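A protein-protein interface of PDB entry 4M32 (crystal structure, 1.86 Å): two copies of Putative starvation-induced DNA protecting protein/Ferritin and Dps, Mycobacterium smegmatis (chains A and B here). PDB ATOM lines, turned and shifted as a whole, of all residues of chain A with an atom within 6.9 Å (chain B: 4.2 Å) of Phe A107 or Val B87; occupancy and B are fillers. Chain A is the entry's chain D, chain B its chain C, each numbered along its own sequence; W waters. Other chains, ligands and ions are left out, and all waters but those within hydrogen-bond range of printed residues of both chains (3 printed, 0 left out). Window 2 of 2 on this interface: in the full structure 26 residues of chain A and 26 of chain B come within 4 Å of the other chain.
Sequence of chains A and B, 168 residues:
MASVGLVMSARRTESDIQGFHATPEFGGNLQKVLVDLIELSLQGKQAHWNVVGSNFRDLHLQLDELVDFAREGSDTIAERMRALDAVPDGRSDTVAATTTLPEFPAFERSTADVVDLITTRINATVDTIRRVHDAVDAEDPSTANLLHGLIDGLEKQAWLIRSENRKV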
ATOM      1  N   GLN A  46     -15.832  -5.427 -12.933  1.00  0.00           N
ATOM      2  CA  GLN A  46     -17.069  -6.201 -12.784  1.00  0.00           C
ATOM      3  C   GLN A  46     -18.287  -5.270 -12.665  1.00  0.00           C
ATOM      4  O   GLN A  46     -19.295  -5.473 -13.344  1.00  0.00           O
ATOM      5  CB  GLN A  46     -16.979  -7.146 -11.578  1.00  0.00           C
ATOM      6  CG  GLN A  46     -18.220  -8.022 -11.348  1.00  0.00           C
ATOM      7  CD  GLN A  46     -18.308  -9.231 -12.277  1.00  0.00           C
ATOM      8  OE1 GLN A  46     -17.388  -9.523 -13.041  1.00  0.00           O
ATOM      9  NE2 GLN A  46     -19.427  -9.942 -12.206  1.00  0.00           N
ATOM     10  N   ASN A  50     -21.374  -4.553 -15.425  1.00  0.00           N
ATOM     11  CA  ASN A  50     -22.677  -5.096 -15.028  1.00  0.00           C
ATOM     12  C   ASN A  50     -23.666  -4.126 -14.390  1.00  0.00           C
ATOM     13  O   ASN A  50     -24.798  -4.510 -14.072  1.00  0.00           O
ATOM     14  CB  ASN A  50     -22.476  -6.315 -14.121  1.00  0.00           C
ATOM     15  CG  ASN A  50     -21.917  -7.503 -14.867  1.00  0.00           C
ATOM     16  OD1 ASN A  50     -22.077  -7.619 -16.084  1.00  0.00           O
ATOM     17  ND2 ASN A  50     -21.259  -8.399 -14.144  1.00  0.00           N
ATOM     18  N   VAL A  51     -23.253  -2.876 -14.213  1.00  0.00           N
ATOM     19  CA  VAL A  51     -24.140  -1.853 -13.661  1.00  0.00           C
ATOM     20  C   VAL A  51     -25.257  -1.522 -14.658  1.00  0.00           C
ATOM     21  O   VAL A  51     -25.015  -1.398 -15.858  1.00  0.00           O
ATOM     22  CB  VAL A  51     -23.359  -0.573 -13.226  1.00  0.00           C
ATOM     23  CG1 VAL A  51     -22.770   0.173 -14.429  1.00  0.00           C
ATOM     24  CG2 VAL A  51     -24.240   0.343 -12.391  1.00  0.00           C
ATOM     25  N   PHE A 104     -17.552  -9.051  -4.364  1.00  0.00           N
ATOM     26  CA  PHE A 104     -18.536  -8.382  -5.206  1.00  0.00           C
ATOM     27  C   PHE A 104     -19.562  -9.417  -5.655  1.00  0.00           C
ATOM     28  O   PHE A 104     -19.187 -10.531  -6.025  1.00  0.00           O
ATOM     29  CB  PHE A 104     -17.881  -7.714  -6.425  1.00  0.00           C
ATOM     30  CG  PHE A 104     -18.735  -6.651  -7.060  1.00  0.00           C
ATOM     31  CD1 PHE A 104     -18.761  -5.360  -6.543  1.00  0.00           C
ATOM     32  CD2 PHE A 104     -19.526  -6.944  -8.164  1.00  0.00           C
ATOM     33  CE1 PHE A 104     -19.563  -4.373  -7.121  1.00  0.00           C
ATOM     34  CE2 PHE A 104     -20.329  -5.970  -8.749  1.00  0.00           C
ATOM     35  CZ  PHE A 104     -20.350  -4.682  -8.221  1.00  0.00           C
ATOM     36  N   PRO A 105     -20.860  -9.064  -5.609  1.00  0.00           N
ATOM     37  CA  PRO A 105     -21.887 -10.016  -6.030  1.00  0.00           C
ATOM     38  C   PRO A 105     -21.902 -10.241  -7.544  1.00  0.00           C
ATOM     39  O   PRO A 105     -21.450  -9.382  -8.310  1.00  0.00           O
ATOM     40  CB  PRO A 105     -23.189  -9.351  -5.575  1.00  0.00           C
ATOM     41  CG  PRO A 105     -22.880  -7.895  -5.555  1.00  0.00           C
ATOM     42  CD  PRO A 105     -21.443  -7.798  -5.126  1.00  0.00           C
ATOM     43  N   ALA A 106     -22.417 -11.395  -7.958  1.00  0.00           N
ATOM     44  CA  ALA A 106     -22.552 -11.728  -9.371  1.00  0.00           C
ATOM     45  C   ALA A 106     -23.746 -11.010  -9.999  1.00  0.00           C
ATOM     46  O   ALA A 106     -24.524 -10.359  -9.300  1.00  0.00           O
ATOM     47  CB  ALA A 106     -22.687 -13.243  -9.541  1.00  0.00           C
ATOM     48  N   PHE A 107     -23.865 -11.133 -11.323  1.00  0.00           N
ATOM     49  CA  PHE A 107     -25.021 -10.657 -12.104  1.00  0.00           C
ATOM     50  C   PHE A 107     -25.120  -9.133 -12.251  1.00  0.00           C
ATOM     51  O   PHE A 107     -24.292  -8.388 -11.723  1.00  0.00           O
ATOM     52  CB  PHE A 107     -26.345 -11.237 -11.571  1.00  0.00           C
ATOM     53  CG  PHE A 107     -26.279 -12.703 -11.234  1.00  0.00           C
ATOM     54  CD1 PHE A 107     -25.913 -13.641 -12.198  1.00  0.00           C
ATOM     55  CD2 PHE A 107     -26.586 -13.144  -9.950  1.00  0.00           C
ATOM     56  CE1 PHE A 107     -25.846 -14.999 -11.884  1.00  0.00           C
ATOM     57  CE2 PHE A 107     -26.526 -14.500  -9.627  1.00  0.00           C
ATOM     58  CZ  PHE A 107     -26.156 -15.427 -10.599  1.00  0.00           C
ATOM     59  N   GLU A 108     -26.131  -8.692 -13.000  1.00  0.00           N
ATOM     60  CA  GLU A 108     -26.446  -7.271 -13.145  1.00  0.00           C
ATOM     61  C   GLU A 108     -26.851  -6.678 -11.801  1.00  0.00           C
ATOM     62  O   GLU A 108     -27.567  -7.314 -11.019  1.00  0.00           O
ATOM     63  CB  GLU A 108     -27.574  -7.070 -14.162  1.00  0.00           C
ATOM     64  CG  GLU A 108     -27.196  -7.417 -15.600  1.00  0.00           C
ATOM     65  CD  GLU A 108     -28.392  -7.411 -16.542  1.00  0.00           C
ATOM     66  OE1 GLU A 108     -29.413  -8.062 -16.223  1.00  0.00           O
ATOM     67  OE2 GLU A 108     -28.309  -6.763 -17.607  1.00  0.00           O
ATOM     68  N   ARG A 109     -26.369  -5.469 -11.524  1.00  0.00           N
ATOM     69  CA  ARG A 109     -26.710  -4.766 -10.288  1.00  0.00           C
ATOM     70  C   ARG A 109     -27.157  -3.352 -10.628  1.00  0.00           C
ATOM     71  O   ARG A 109     -26.648  -2.748 -11.574  1.00  0.00           O
ATOM     72  CB  ARG A 109     -25.521  -4.710  -9.313  1.00  0.00           C
ATOM     73  CG  ARG A 109     -24.643  -5.968  -9.200  1.00  0.00           C
ATOM     74  CD  ARG A 109     -25.396  -7.208  -8.715  1.00  0.00           C
ATOM     75  NE  ARG A 109     -25.962  -7.062  -7.378  1.00  0.00           N
ATOM     76  CZ  ARG A 109     -26.450  -8.067  -6.653  1.00  0.00           C
ATOM     77  NH1 ARG A 109     -26.438  -9.309  -7.122  1.00  0.00           N
ATOM     78  NH2 ARG A 109     -26.944  -7.829  -5.446  1.00  0.00           N
ATOM     79  N   MET B  81     -20.395  -9.331 -24.543  1.00  0.00           N
ATOM     80  CA  MET B  81     -21.348 -10.101 -23.741  1.00  0.00           C
ATOM     81  C   MET B  81     -22.519  -9.216 -23.310  1.00  0.00           C
ATOM     82  O   MET B  81     -23.680  -9.577 -23.512  1.00  0.00           O
ATOM     83  CB  MET B  81     -20.658 -10.731 -22.526  1.00  0.00           C
ATOM     84  CG  MET B  81     -19.660 -11.833 -22.881  1.00  0.00           C
ATOM     85  SD  MET B  81     -18.730 -12.468 -21.470  1.00  0.00           S
ATOM     86  CE  MET B  81     -19.969 -13.531 -20.719  1.00  0.00           C
ATOM     87  N   ARG B  82     -22.212  -8.044 -22.751  1.00  0.00           N
ATOM     88  CA  ARG B  82     -23.252  -7.099 -22.334  1.00  0.00           C
ATOM     89  C   ARG B  82     -24.166  -6.689 -23.489  1.00  0.00           C
ATOM     90  O   ARG B  82     -25.388  -6.638 -23.325  1.00  0.00           O
ATOM     91  CB  ARG B  82     -22.649  -5.860 -21.659  1.00  0.00           C
ATOM     92  CG  ARG B  82     -21.898  -6.141 -20.355  1.00  0.00           C
ATOM     93  CD  ARG B  82     -22.760  -6.860 -19.301  1.00  0.00           C
ATOM     94  NE  ARG B  82     -23.848  -6.023 -18.801  1.00  0.00           N
ATOM     95  CZ  ARG B  82     -25.133  -6.374 -18.780  1.00  0.00           C
ATOM     96  NH1 ARG B  82     -26.033  -5.524 -18.305  1.00  0.00           N
ATOM     97  NH2 ARG B  82     -25.521  -7.569 -19.215  1.00  0.00           N
ATOM     98  N   ALA B  86     -25.664 -11.017 -22.303  1.00  0.00           N
ATOM     99  CA  ALA B  86     -24.946 -11.970 -21.456  1.00  0.00           C
ATOM    100  C   ALA B  86     -24.283 -11.229 -20.299  1.00  0.00           C
ATOM    101  O   ALA B  86     -24.107 -10.006 -20.357  1.00  0.00           O
ATOM    102  CB  ALA B  86     -23.910 -12.750 -22.267  1.00  0.00           C
ATOM    103  N   VAL B  87     -23.932 -11.963 -19.246  1.00  0.00           N
ATOM    104  CA  VAL B  87     -23.386 -11.352 -18.036  1.00  0.00           C
ATOM    105  C   VAL B  87     -21.997 -11.917 -17.709  1.00  0.00           C
ATOM    106  O   VAL B  87     -21.877 -13.080 -17.301  1.00  0.00           O
ATOM    107  CB  VAL B  87     -24.346 -11.516 -16.820  1.00  0.00           C
ATOM    108  CG1 VAL B  87     -23.808 -10.767 -15.608  1.00  0.00           C
ATOM    109  CG2 VAL B  87     -25.752 -11.022 -17.159  1.00  0.00           C
ATOM    110  N   PRO B  88     -20.942 -11.095 -17.887  1.00  0.00           N
ATOM    111  CA  PRO B  88     -19.580 -11.526 -17.589  1.00  0.00           C
ATOM    112  C   PRO B  88     -19.343 -11.713 -16.094  1.00  0.00           C
ATOM    113  O   PRO B  88     -20.034 -11.111 -15.269  1.00  0.00           O
ATOM    114  CB  PRO B  88     -18.723 -10.369 -18.117  1.00  0.00           C
ATOM    115  CG  PRO B  88     -19.606  -9.190 -18.065  1.00  0.00           C
ATOM    116  CD  PRO B  88     -20.970  -9.714 -18.406  1.00  0.00           C
ATOM    117  N   ASP B  89     -18.383 -12.571 -15.765  1.00  0.00           N
ATOM    118  CA  ASP B  89     -17.897 -12.705 -14.402  1.00  0.00           C
ATOM    119  C   ASP B  89     -16.372 -12.688 -14.433  1.00  0.00           C
ATOM    120  O   ASP B  89     -15.729 -13.693 -14.750  1.00  0.00           O
ATOM    121  CB  ASP B  89     -18.435 -13.981 -13.744  1.00  0.00           C
ATOM    122  CG  ASP B  89     -18.055 -14.091 -12.273  1.00  0.00           C
ATOM    123  OD1 ASP B  89     -17.393 -13.173 -11.740  1.00  0.00           O
ATOM    124  OD2 ASP B  89     -18.429 -15.106 -11.644  1.00  0.00           O
HETATM  125  O   HOH W   1     -21.567 -12.177 -12.927  1.00  0.00           O
HETATM  126  O   HOH W   2     -28.231  -8.098 -19.968  1.00  0.00           O
HETATM  127  O   HOH W   3     -24.456  -3.000 -17.958  1.00  0.00           O
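No position is printed for both chains.
Printed residues of chain B that touch a printed residue of chain A: Arg B82, Val B87, Pro B88 and Asp B89. Hydrophobic or aromatic side chains of chain B within 4 Å of the printed part of chain A: Val B87 and Pro B88. Printed residues of chain A that touch a printed residue of chain B: Gln A46, Asn A50, Phe A107 and Glu A108. Among the printed residues, Asp or Glu carboxylates within 4 Å of a Lys or Arg side-chain nitrogen of the other chain: Glu A108 with Arg B82.
The guanidinium group (NH2) of Arg B82 lies within hydrogen-bond range of the backbone carbonyl oxygen (O) of Ala B86 (3.0 Å). The side-chain amide nitrogen of Gln A46 sits close to the side-chain amide nitrogen of Asn A50. The backbone carbonyl oxygen (O) of Asn A50 lies within hydrogen-bond range of the backbone NH (N) of Arg A109 (3.1 Å).
Among the printed residues, merely in contact across the chains: Asn A50 with Arg B82, Gln A46 with Asp B89, Asn A50 with Val B87 and Phe A107 with Val B87.
NH1 of Arg B82 lies within salt-bridge range of OE2 of Glu A108, at 2.7 Å. The backbone carbonyl oxygen (O) of Pro B88 sits at hydrogen-bond distance from the side-chain amide nitrogen (NE2) of Gln A46 (3.3 Å). The backbone carbonyl oxygen of Pro B88 sits at hydrogen-bond distance from the side-chain amide nitrogen of Asn A50, at 3.2 Å.
Of the printed residues of chain B, Gln A46 touches Pro B88 (3.3 Å) and Asp B89 (3.5 Å). Printed residues of chain B within 4 Å of Asn A50: Arg B82, Val B87 and Pro B88. Phe A107 touches just one residue of chain B: Val B87. Of the printed residues of chain B, Glu A108 touches Arg B82 (2.7 Å). Of the printed residues of chain A, Arg B82 touches Asn A50 and Glu A108. Val B87 touches two residues of chain A. Of the printed residues of chain A, Asp B89 touches Gln A46 (3.5 Å). The nearest printed residue of chain B that does not touch Phe A107 is Pro B88 (5.5 Å). The nearest residue of chain A that does not touch Val B87 is Glu A108 (4.1 Å).
Water W3 lies within hydrogen-bond range of the backbone carbonyl oxygen (O) of Val A51 (2.7 Å) and the guanidinium group (NH1) of Arg B82 (3.0 Å). Water W2 lies within hydrogen-bond range of OE2 of Glu A108 (2.7 Å) and NH2 of Arg B82 (2.9 Å). Water W1 lies within hydrogen-bond range of N of Phe A107 (3.0 Å), O of Pro B88 (3.0 Å) and NE2 of Gln A46 (3.2 Å).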
